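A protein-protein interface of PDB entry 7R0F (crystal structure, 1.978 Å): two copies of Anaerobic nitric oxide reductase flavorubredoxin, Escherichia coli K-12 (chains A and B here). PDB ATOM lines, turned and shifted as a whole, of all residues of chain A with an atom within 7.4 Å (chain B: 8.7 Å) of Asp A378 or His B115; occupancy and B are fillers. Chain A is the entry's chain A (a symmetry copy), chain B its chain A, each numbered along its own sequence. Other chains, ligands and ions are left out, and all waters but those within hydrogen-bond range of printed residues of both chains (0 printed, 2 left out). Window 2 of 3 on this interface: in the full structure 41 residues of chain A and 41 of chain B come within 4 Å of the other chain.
The side-chain carboxylate (OD2) of Asp B108 is in hydrogen-bond range of the indole nitrogen (NE1) of Trp A375 (2.9 Å).
O of Arg A376 sits close to NE2 of His B115, 3.3 Å away.
O of Gly B112 sits at hydrogen-bond distance from N of Arg A376 (3.2 Å).
The side-chain amino group of Lys A374 is in salt-bridge range of the side-chain carboxylate of Asp B108 (2.9 Å).
A ring nitrogen (ND1) of His B115 is in hydrogen-bond range of the backbone carbonyl oxygen (O) of Asn B111 (3.0 Å).
A ring nitrogen (ND1) of His B113 is in hydrogen-bond range of the backbone carbonyl oxygen (O) of Ser B109 (2.6 Å).
OD1 of Asp A378 sits at hydrogen-bond distance from N of Asp A380 (3.2 Å).
OD1 of Asp A378 is in hydrogen-bond range of N of Ala A381, 2.9 Å away.
The guanidinium group (NH1) of Arg A376 is in hydrogen-bond range of the side-chain sulfur (SD) of Met A267 (3.4 Å).
Among the printed residues, pairs that only touch across the chains: Trp A375 with Ser B109, Trp A375 with Gly B112, Trp A375 with His B113, Arg A376 with His B113, Pro A377 with His B115 and Asp A378 with His B115.
Of chain B, only His B115 (3.5 Å) comes within 4 Å of Asp A378.
Printed residues of chain A within 4 Å of His B115: Arg A376, Pro A377 and Asp A378.
Of the printed residues of chain A, Gly B112 touches Trp A375 (3.4 Å) and Arg A376 (3.2 Å).
Of the printed residues of chain B, Lys A374 touches Asp B108 (2.9 Å).
Printed residues of chain A within 4 Å of Asp B108: Lys A374 (2.9 Å) and Trp A375 (2.9 Å).
Printed residues of chain B within 4 Å of Trp A375: Asp B108, Ser B109, Gly B112 and His B113.
The nearest printed residue of chain A that does not touch His B115 is Gln A379 (5.4 Å).
Hydrophobic or aromatic side chains of chain A that line the printed part of chain B: Trp A375.
Of the 15 printed residues of chain B, 5 touch a printed residue of chain A.
Hydrophobic or aromatic side chains of chain B that line the printed part of chain A: His B113 and His B115.
Among the printed residues, 10 pairs touch across the chains.
Among the printed residues, Asp or Glu carboxylates within 4 Å of a Lys or Arg side-chain nitrogen of the other chain: Lys A374 with Asp B108 (2.9 Å).
No position is printed for both chains.
Of the 10 pairs that touch across the chains among the printed residues, none has its exchanged pair printed and touching as well.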
ATOM      1  N   MET A 267       4.615 -20.522 -31.282  1.00  0.00           N
ATOM      2  CA  MET A 267       3.532 -21.496 -31.322  1.00  0.00           C
ATOM      3  C   MET A 267       2.528 -21.158 -32.417  1.00  0.00           C
ATOM      4  O   MET A 267       1.985 -22.050 -33.068  1.00  0.00           O
ATOM      5  CB  MET A 267       2.830 -21.573 -29.965  1.00  0.00           C
ATOM      6  CG  MET A 267       3.686 -22.179 -28.864  1.00  0.00           C
ATOM      7  SD  MET A 267       2.846 -22.223 -27.272  1.00  0.00           S
ATOM      8  CE  MET A 267       1.479 -23.323 -27.636  1.00  0.00           C
ATOM      9  N   ALA A 373      -3.420 -13.141 -31.108  1.00  0.00           N
ATOM     10  CA  ALA A 373      -3.739 -14.056 -30.020  1.00  0.00           C
ATOM     11  C   ALA A 373      -3.275 -13.470 -28.693  1.00  0.00           C
ATOM     12  O   ALA A 373      -2.318 -12.698 -28.650  1.00  0.00           O
ATOM     13  CB  ALA A 373      -3.101 -15.415 -30.258  1.00  0.00           C
ATOM     14  N   LYS A 374      -3.955 -13.837 -27.614  1.00  0.00           N
ATOM     15  CA  LYS A 374      -3.615 -13.325 -26.293  1.00  0.00           C
ATOM     16  C   LYS A 374      -2.840 -14.364 -25.492  1.00  0.00           C
ATOM     17  O   LYS A 374      -3.288 -15.502 -25.347  1.00  0.00           O
ATOM     18  CB  LYS A 374      -4.881 -12.907 -25.542  1.00  0.00           C
ATOM     19  CG  LYS A 374      -4.639 -11.952 -24.387  1.00  0.00           C
ATOM     20  CD  LYS A 374      -5.944 -11.602 -23.688  1.00  0.00           C
ATOM     21  CE  LYS A 374      -5.720 -10.581 -22.586  1.00  0.00           C
ATOM     22  NZ  LYS A 374      -6.968 -10.293 -21.827  1.00  0.00           N
ATOM     23  N   TRP A 375      -1.676 -13.961 -24.985  1.00  0.00           N
ATOM     24  CA  TRP A 375      -0.796 -14.838 -24.213  1.00  0.00           C
ATOM     25  C   TRP A 375      -0.456 -16.119 -24.977  1.00  0.00           C
ATOM     26  O   TRP A 375      -0.250 -16.092 -26.192  1.00  0.00           O
ATOM     27  CB  TRP A 375      -1.426 -15.185 -22.860  1.00  0.00           C
ATOM     28  CG  TRP A 375      -1.792 -13.988 -22.023  1.00  0.00           C
ATOM     29  CD1 TRP A 375      -3.048 -13.605 -21.645  1.00  0.00           C
ATOM     30  CD2 TRP A 375      -0.892 -13.022 -21.464  1.00  0.00           C
ATOM     31  NE1 TRP A 375      -2.985 -12.464 -20.880  1.00  0.00           N
ATOM     32  CE2 TRP A 375      -1.673 -12.084 -20.756  1.00  0.00           C
ATOM     33  CE3 TRP A 375       0.496 -12.858 -21.491  1.00  0.00           C
ATOM     34  CZ2 TRP A 375      -1.112 -11.001 -20.081  1.00  0.00           C
ATOM     35  CZ3 TRP A 375       1.053 -11.781 -20.822  1.00  0.00           C
ATOM     36  CH2 TRP A 375       0.251 -10.868 -20.127  1.00  0.00           C
ATOM     37  N   ARG A 376      -0.402 -17.236 -24.258  1.00  0.00           N
ATOM     38  CA  ARG A 376      -0.119 -18.530 -24.866  1.00  0.00           C
ATOM     39  C   ARG A 376      -1.380 -19.122 -25.486  1.00  0.00           C
ATOM     40  O   ARG A 376      -2.400 -19.258 -24.813  1.00  0.00           O
ATOM     41  CB  ARG A 376       0.464 -19.495 -23.831  1.00  0.00           C
ATOM     42  CG  ARG A 376       0.714 -20.901 -24.357  1.00  0.00           C
ATOM     43  CD  ARG A 376       1.274 -21.809 -23.271  1.00  0.00           C
ATOM     44  NE  ARG A 376       2.608 -21.399 -22.844  1.00  0.00           N
ATOM     45  CZ  ARG A 376       3.732 -21.985 -23.242  1.00  0.00           C
ATOM     46  NH1 ARG A 376       3.686 -23.012 -24.079  1.00  0.00           N
ATOM     47  NH2 ARG A 376       4.904 -21.547 -22.801  1.00  0.00           N
ATOM     48  N   PRO A 377      -1.313 -19.478 -26.778  1.00  0.00           N
ATOM     49  CA  PRO A 377      -2.462 -20.059 -27.482  1.00  0.00           C
ATOM     50  C   PRO A 377      -2.847 -21.434 -26.944  1.00  0.00           C
ATOM     51  O   PRO A 377      -2.006 -22.332 -26.915  1.00  0.00           O
ATOM     52  CB  PRO A 377      -1.973 -20.169 -28.932  1.00  0.00           C
ATOM     53  CG  PRO A 377      -0.773 -19.278 -29.019  1.00  0.00           C
ATOM     54  CD  PRO A 377      -0.149 -19.313 -27.663  1.00  0.00           C
ATOM     55  N   ASP A 378      -4.098 -21.596 -26.521  1.00  0.00           N
ATOM     56  CA  ASP A 378      -4.593 -22.915 -26.148  1.00  0.00           C
ATOM     57  C   ASP A 378      -5.011 -23.673 -27.405  1.00  0.00           C
ATOM     58  O   ASP A 378      -4.750 -23.219 -28.518  1.00  0.00           O
ATOM     59  CB  ASP A 378      -5.757 -22.815 -25.153  1.00  0.00           C
ATOM     60  CG  ASP A 378      -6.864 -21.885 -25.623  1.00  0.00           C
ATOM     61  OD1 ASP A 378      -7.021 -21.688 -26.845  1.00  0.00           O
ATOM     62  OD2 ASP A 378      -7.589 -21.350 -24.757  1.00  0.00           O
ATOM     63  N   GLN A 379      -5.659 -24.819 -27.226  1.00  0.00           N
ATOM     64  CA  GLN A 379      -6.045 -25.659 -28.355  1.00  0.00           C
ATOM     65  C   GLN A 379      -7.022 -24.952 -29.290  1.00  0.00           C
ATOM     66  O   GLN A 379      -6.976 -25.145 -30.504  1.00  0.00           O
ATOM     67  CB  GLN A 379      -6.650 -26.974 -27.859  1.00  0.00           C
ATOM     68  CG  GLN A 379      -5.630 -27.922 -27.252  1.00  0.00           C
ATOM     69  CD  GLN A 379      -4.496 -28.245 -28.210  1.00  0.00           C
ATOM     70  OE1 GLN A 379      -4.716 -28.807 -29.284  1.00  0.00           O
ATOM     71  NE2 GLN A 379      -3.276 -27.885 -27.827  1.00  0.00           N
ATOM     72  N   ASP A 380      -7.898 -24.128 -28.723  1.00  0.00           N
ATOM     73  CA  ASP A 380      -8.864 -23.378 -29.517  1.00  0.00           C
ATOM     74  C   ASP A 380      -8.169 -22.295 -30.337  1.00  0.00           C
ATOM     75  O   ASP A 380      -8.479 -22.093 -31.511  1.00  0.00           O
ATOM     76  CB  ASP A 380      -9.930 -22.752 -28.615  1.00  0.00           C
ATOM     77  CG  ASP A 380     -10.704 -23.786 -27.824  1.00  0.00           C
ATOM     78  OD1 ASP A 380     -10.949 -24.887 -28.361  1.00  0.00           O
ATOM     79  OD2 ASP A 380     -11.065 -23.500 -26.662  1.00  0.00           O
ATOM     80  N   ALA A 381      -7.228 -21.601 -29.706  1.00  0.00           N
ATOM     81  CA  ALA A 381      -6.483 -20.537 -30.367  1.00  0.00           C
ATOM     82  C   ALA A 381      -5.585 -21.092 -31.470  1.00  0.00           C
ATOM     83  O   ALA A 381      -5.409 -20.462 -32.512  1.00  0.00           O
ATOM     84  CB  ALA A 381      -5.661 -19.760 -29.355  1.00  0.00           C
ATOM     85  N   LEU A 382      -5.020 -22.272 -31.235  1.00  0.00           N
ATOM     86  CA  LEU A 382      -4.155 -22.911 -32.222  1.00  0.00           C
ATOM     87  C   LEU A 382      -4.939 -23.357 -33.452  1.00  0.00           C
ATOM     88  O   LEU A 382      -4.390 -23.421 -34.553  1.00  0.00           O
ATOM     89  CB  LEU A 382      -3.422 -24.104 -31.604  1.00  0.00           C
ATOM     90  CG  LEU A 382      -2.298 -23.770 -30.623  1.00  0.00           C
ATOM     91  CD1 LEU A 382      -1.678 -25.041 -30.063  1.00  0.00           C
ATOM     92  CD2 LEU A 382      -1.241 -22.908 -31.293  1.00  0.00           C
ATOM     93  N   LYS A 383      -6.217 -23.670 -33.259  1.00  0.00           N
ATOM     94  CA  LYS A 383      -7.100 -23.991 -34.376  1.00  0.00           C
ATOM     95  C   LYS A 383      -7.303 -22.766 -35.260  1.00  0.00           C
ATOM     96  O   LYS A 383      -7.323 -22.871 -36.487  1.00  0.00           O
ATOM     97  CB  LYS A 383      -8.449 -24.511 -33.877  1.00  0.00           C
ATOM     98  CG  LYS A 383      -8.396 -25.892 -33.246  1.00  0.00           C
ATOM     99  CD  LYS A 383      -9.789 -26.394 -32.900  1.00  0.00           C
ATOM    100  CE  LYS A 383      -9.728 -27.703 -32.132  1.00  0.00           C
ATOM    101  NZ  LYS A 383      -9.014 -28.762 -32.898  1.00  0.00           N
ATOM    102  N   LEU A 384      -7.461 -21.608 -34.625  1.00  0.00           N
ATOM    103  CA  LEU A 384      -7.610 -20.348 -35.346  1.00  0.00           C
ATOM    104  C   LEU A 384      -6.343 -20.021 -36.130  1.00  0.00           C
ATOM    105  O   LEU A 384      -6.411 -19.527 -37.255  1.00  0.00           O
ATOM    106  CB  LEU A 384      -7.944 -19.209 -34.379  1.00  0.00           C
ATOM    107  CG  LEU A 384      -9.263 -19.321 -33.611  1.00  0.00           C
ATOM    108  CD1 LEU A 384      -9.426 -18.156 -32.645  1.00  0.00           C
ATOM    109  CD2 LEU A 384     -10.444 -19.395 -34.570  1.00  0.00           C
ATOM    110  N   CYS A 385      -5.190 -20.299 -35.529  1.00  0.00           N
ATOM    111  CA  CYS A 385      -3.908 -20.079 -36.190  1.00  0.00           C
ATOM    112  C   CYS A 385      -3.755 -21.041 -37.359  1.00  0.00           C
ATOM    113  O   CYS A 385      -3.250 -20.675 -38.421  1.00  0.00           O
ATOM    114  CB  CYS A 385      -2.748 -20.254 -35.208  1.00  0.00           C
ATOM    115  SG  CYS A 385      -2.764 -19.123 -33.800  1.00  0.00           S
ATOM    116  N   ARG A 386      -4.198 -22.277 -37.152  1.00  0.00           N
ATOM    117  CA  ARG A 386      -4.143 -23.294 -38.192  1.00  0.00           C
ATOM    118  C   ARG A 386      -5.094 -22.934 -39.327  1.00  0.00           C
ATOM    119  O   ARG A 386      -4.801 -23.173 -40.498  1.00  0.00           O
ATOM    120  CB  ARG A 386      -4.488 -24.672 -37.618  1.00  0.00           C
ATOM    121  CG  ARG A 386      -3.809 -25.832 -38.332  1.00  0.00           C
ATOM    122  CD  ARG A 386      -3.548 -27.003 -37.385  1.00  0.00           C
ATOM    123  NE  ARG A 386      -4.767 -27.477 -36.735  1.00  0.00           N
ATOM    124  CZ  ARG A 386      -4.995 -27.393 -35.427  1.00  0.00           C
ATOM    125  NH1 ARG A 386      -4.095 -26.832 -34.630  1.00  0.00           N
ATOM    126  NH2 ARG A 386      -6.129 -27.852 -34.914  1.00  0.00           N
ATOM    127  N   THR B  89       1.987 -24.783 -12.770  1.00  0.00           N
ATOM    128  CA  THR B  89       1.267 -25.960 -13.253  1.00  0.00           C
ATOM    129  C   THR B  89       1.792 -27.237 -12.603  1.00  0.00           C
ATOM    130  O   THR B  89       1.016 -28.085 -12.160  1.00  0.00           O
ATOM    131  CB  THR B  89       1.364 -26.091 -14.788  1.00  0.00           C
ATOM    132  OG1 THR B  89       0.662 -25.007 -15.407  1.00  0.00           O
ATOM    133  CG2 THR B  89       0.756 -27.406 -15.256  1.00  0.00           C
ATOM    134  N   ILE B 107      -5.435 -13.198 -12.878  1.00  0.00           N
ATOM    135  CA  ILE B 107      -6.241 -14.346 -13.280  1.00  0.00           C
ATOM    136  C   ILE B 107      -6.192 -14.507 -14.796  1.00  0.00           C
ATOM    137  O   ILE B 107      -6.102 -15.620 -15.314  1.00  0.00           O
ATOM    138  CB  ILE B 107      -7.706 -14.210 -12.818  1.00  0.00           C
ATOM    139  CG1 ILE B 107      -7.785 -14.210 -11.290  1.00  0.00           C
ATOM    140  CG2 ILE B 107      -8.558 -15.339 -13.378  1.00  0.00           C
ATOM    141  CD1 ILE B 107      -9.200 -14.235 -10.762  1.00  0.00           C
ATOM    142  N   ASP B 108      -6.227 -13.382 -15.499  1.00  0.00           N
ATOM    143  CA  ASP B 108      -6.146 -13.384 -16.953  1.00  0.00           C
ATOM    144  C   ASP B 108      -4.766 -13.823 -17.441  1.00  0.00           C
ATOM    145  O   ASP B 108      -4.653 -14.563 -18.417  1.00  0.00           O
ATOM    146  CB  ASP B 108      -6.482 -11.996 -17.504  1.00  0.00           C
ATOM    147  CG  ASP B 108      -6.366 -11.926 -19.013  1.00  0.00           C
ATOM    148  OD1 ASP B 108      -7.343 -12.281 -19.704  1.00  0.00           O
ATOM    149  OD2 ASP B 108      -5.296 -11.513 -19.506  1.00  0.00           O
ATOM    150  N   SER B 109      -3.720 -13.369 -16.758  1.00  0.00           N
ATOM    151  CA  SER B 109      -2.354 -13.686 -17.167  1.00  0.00           C
ATOM    152  C   SER B 109      -1.952 -15.106 -16.763  1.00  0.00           C
ATOM    153  O   SER B 109      -1.258 -15.794 -17.511  1.00  0.00           O
ATOM    154  CB  SER B 109      -1.367 -12.675 -16.578  1.00  0.00           C
ATOM    155  OG  SER B 109      -1.446 -12.643 -15.165  1.00  0.00           O
ATOM    156  N   ILE B 110      -2.385 -15.541 -15.582  1.00  0.00           N
ATOM    157  CA  ILE B 110      -2.110 -16.904 -15.132  1.00  0.00           C
ATOM    158  C   ILE B 110      -2.800 -17.916 -16.044  1.00  0.00           C
ATOM    159  O   ILE B 110      -2.160 -18.829 -16.566  1.00  0.00           O
ATOM    160  CB  ILE B 110      -2.561 -17.134 -13.675  1.00  0.00           C
ATOM    161  CG1 ILE B 110      -1.661 -16.361 -12.709  1.00  0.00           C
ATOM    162  CG2 ILE B 110      -2.518 -18.612 -13.331  1.00  0.00           C
ATOM    163  CD1 ILE B 110      -2.151 -16.366 -11.277  1.00  0.00           C
ATOM    164  N   ASN B 111      -4.105 -17.744 -16.235  1.00  0.00           N
ATOM    165  CA  ASN B 111      -4.867 -18.605 -17.135  1.00  0.00           C
ATOM    166  C   ASN B 111      -4.365 -18.516 -18.570  1.00  0.00           C
ATOM    167  O   ASN B 111      -4.424 -19.490 -19.319  1.00  0.00           O
ATOM    168  CB  ASN B 111      -6.354 -18.252 -17.087  1.00  0.00           C
ATOM    169  CG  ASN B 111      -7.001 -18.633 -15.771  1.00  0.00           C
ATOM    170  OD1 ASN B 111      -6.507 -19.502 -15.051  1.00  0.00           O
ATOM    171  ND2 ASN B 111      -8.115 -17.986 -15.450  1.00  0.00           N
ATOM    172  N   GLY B 112      -3.869 -17.341 -18.946  1.00  0.00           N
ATOM    173  CA  GLY B 112      -3.335 -17.124 -20.277  1.00  0.00           C
ATOM    174  C   GLY B 112      -2.143 -18.006 -20.597  1.00  0.00           C
ATOM    175  O   GLY B 112      -1.937 -18.390 -21.750  1.00  0.00           O
ATOM    176  N   HIS B 113      -1.354 -18.327 -19.577  1.00  0.00           N
ATOM    177  CA  HIS B 113      -0.173 -19.164 -19.760  1.00  0.00           C
ATOM    178  C   HIS B 113      -0.426 -20.635 -19.428  1.00  0.00           C
ATOM    179  O   HIS B 113       0.052 -21.527 -20.130  1.00  0.00           O
ATOM    180  CB  HIS B 113       0.987 -18.645 -18.905  1.00  0.00           C
ATOM    181  CG  HIS B 113       1.481 -17.290 -19.307  1.00  0.00           C
ATOM    182  ND1 HIS B 113       1.017 -16.127 -18.731  1.00  0.00           N
ATOM    183  CD2 HIS B 113       2.404 -16.914 -20.224  1.00  0.00           C
ATOM    184  CE1 HIS B 113       1.632 -15.093 -19.276  1.00  0.00           C
ATOM    185  NE2 HIS B 113       2.477 -15.543 -20.186  1.00  0.00           N
ATOM    186  N   HIS B 114      -1.179 -20.884 -18.360  1.00  0.00           N
ATOM    187  CA  HIS B 114      -1.299 -22.233 -17.811  1.00  0.00           C
ATOM    188  C   HIS B 114      -2.569 -22.967 -18.228  1.00  0.00           C
ATOM    189  O   HIS B 114      -2.620 -24.196 -18.174  1.00  0.00           O
ATOM    190  CB  HIS B 114      -1.215 -22.178 -16.285  1.00  0.00           C
ATOM    191  CG  HIS B 114       0.108 -21.701 -15.777  1.00  0.00           C
ATOM    192  ND1 HIS B 114       1.182 -22.545 -15.597  1.00  0.00           N
ATOM    193  CD2 HIS B 114       0.535 -20.466 -15.419  1.00  0.00           C
ATOM    194  CE1 HIS B 114       2.214 -21.853 -15.149  1.00  0.00           C
ATOM    195  NE2 HIS B 114       1.848 -20.589 -15.031  1.00  0.00           N
ATOM    196  N   HIS B 115      -3.587 -22.211 -18.629  1.00  0.00           N
ATOM    197  CA  HIS B 115      -4.850 -22.773 -19.111  1.00  0.00           C
ATOM    198  C   HIS B 115      -5.541 -23.643 -18.066  1.00  0.00           C
ATOM    199  O   HIS B 115      -6.160 -24.651 -18.403  1.00  0.00           O
ATOM    200  CB  HIS B 115      -4.629 -23.595 -20.385  1.00  0.00           C
ATOM    201  CG  HIS B 115      -3.915 -22.851 -21.469  1.00  0.00           C
ATOM    202  ND1 HIS B 115      -3.767 -21.484 -21.460  1.00  0.00           N
ATOM    203  CD2 HIS B 115      -3.308 -23.292 -22.598  1.00  0.00           C
ATOM    204  CE1 HIS B 115      -3.097 -21.109 -22.539  1.00  0.00           C
ATOM    205  NE2 HIS B 115      -2.808 -22.185 -23.242  1.00  0.00           N
ATOM    206  N   HIS B 116      -5.430 -23.256 -16.800  1.00  0.00           N
ATOM    207  CA  HIS B 116      -6.137 -23.956 -15.731  1.00  0.00           C
ATOM    208  C   HIS B 116      -7.025 -23.000 -14.943  1.00  0.00           C
ATOM    209  O   HIS B 116      -6.714 -22.657 -13.803  1.00  0.00           O
ATOM    210  CB  HIS B 116      -5.153 -24.648 -14.787  1.00  0.00           C
ATOM    211  CG  HIS B 116      -4.537 -25.889 -15.352  1.00  0.00           C
ATOM    212  ND1 HIS B 116      -5.186 -27.105 -15.359  1.00  0.00           N
ATOM    213  CD2 HIS B 116      -3.323 -26.108 -15.913  1.00  0.00           C
ATOM    214  CE1 HIS B 116      -4.404 -28.016 -15.910  1.00  0.00           C
ATOM    215  NE2 HIS B 116      -3.268 -27.437 -16.253  1.00  0.00           N
ATOM    216  N   PRO B 117      -8.142 -22.568 -15.549  1.00  0.00           N
ATOM    217  CA  PRO B 117      -9.040 -21.619 -14.884  1.00  0.00           C
ATOM    218  C   PRO B 117      -9.751 -22.226 -13.678  1.00  0.00           C
ATOM    219  O   PRO B 117     -10.342 -21.489 -12.889  1.00  0.00           O
ATOM    220  CB  PRO B 117     -10.045 -21.258 -15.983  1.00  0.00           C
ATOM    221  CG  PRO B 117     -10.050 -22.440 -16.887  1.00  0.00           C
ATOM    222  CD  PRO B 117      -8.645 -22.971 -16.875  1.00  0.00           C
ATOM    223  N   GLU B 118      -9.683 -23.546 -13.532  1.00  0.00           N
ATOM    224  CA  GLU B 118     -10.375 -24.227 -12.442  1.00  0.00           C
ATOM    225  C   GLU B 118      -9.659 -24.052 -11.105  1.00  0.00           C
ATOM    226  O   GLU B 118     -10.203 -24.396 -10.058  1.00  0.00           O
ATOM    227  CB  GLU B 118     -10.536 -25.718 -12.753  1.00  0.00           C
ATOM    228  CG  GLU B 118      -9.269 -26.542 -12.578  1.00  0.00           C
ATOM    229  CD  GLU B 118      -8.345 -26.467 -13.778  1.00  0.00           C
ATOM    230  OE1 GLU B 118      -8.700 -25.793 -14.767  1.00  0.00           O
ATOM    231  OE2 GLU B 118      -7.261 -27.086 -13.729  1.00  0.00           O
ATOM    232  N   TRP B 119      -8.438 -23.524 -11.144  1.00  0.00           N
ATOM    233  CA  TRP B 119      -7.694 -23.228  -9.923  1.00  0.00           C
ATOM    234  C   TRP B 119      -8.461 -22.236  -9.055  1.00  0.00           C
ATOM    235  O   TRP B 119      -9.207 -21.401  -9.564  1.00  0.00           O
ATOM    236  CB  TRP B 119      -6.305 -22.678 -10.254  1.00  0.00           C
ATOM    237  CG  TRP B 119      -5.365 -23.706 -10.809  1.00  0.00           C
ATOM    238  CD1 TRP B 119      -5.512 -25.062 -10.761  1.00  0.00           C
ATOM    239  CD2 TRP B 119      -4.135 -23.459 -11.502  1.00  0.00           C
ATOM    240  NE1 TRP B 119      -4.447 -25.675 -11.378  1.00  0.00           N
ATOM    241  CE2 TRP B 119      -3.588 -24.713 -11.842  1.00  0.00           C
ATOM    242  CE3 TRP B 119      -3.444 -22.300 -11.869  1.00  0.00           C
ATOM    243  CZ2 TRP B 119      -2.384 -24.840 -12.533  1.00  0.00           C
ATOM    244  CZ3 TRP B 119      -2.247 -22.428 -12.552  1.00  0.00           C
ATOM    245  CH2 TRP B 119      -1.729 -23.689 -12.876  1.00  0.00           C
ATOM    246  N   PHE B 121      -8.728 -19.184  -7.452  1.00  0.00           N
ATOM    247  CA  PHE B 121      -8.151 -17.845  -7.391  1.00  0.00           C
ATOM    248  C   PHE B 121      -8.854 -16.966  -6.365  1.00  0.00           C
ATOM    249  O   PHE B 121     -10.070 -17.037  -6.198  1.00  0.00           O
ATOM    250  CB  PHE B 121      -8.211 -17.167  -8.763  1.00  0.00           C
ATOM    251  CG  PHE B 121      -7.375 -17.839  -9.813  1.00  0.00           C
ATOM    252  CD1 PHE B 121      -6.002 -17.662  -9.842  1.00  0.00           C
ATOM    253  CD2 PHE B 121      -7.965 -18.637 -10.780  1.00  0.00           C
ATOM    254  CE1 PHE B 121      -5.230 -18.274 -10.811  1.00  0.00           C
ATOM    255  CE2 PHE B 121      -7.199 -19.252 -11.751  1.00  0.00           C
ATOM    256  CZ  PHE B 121      -5.831 -19.070 -11.767  1.00  0.00           C
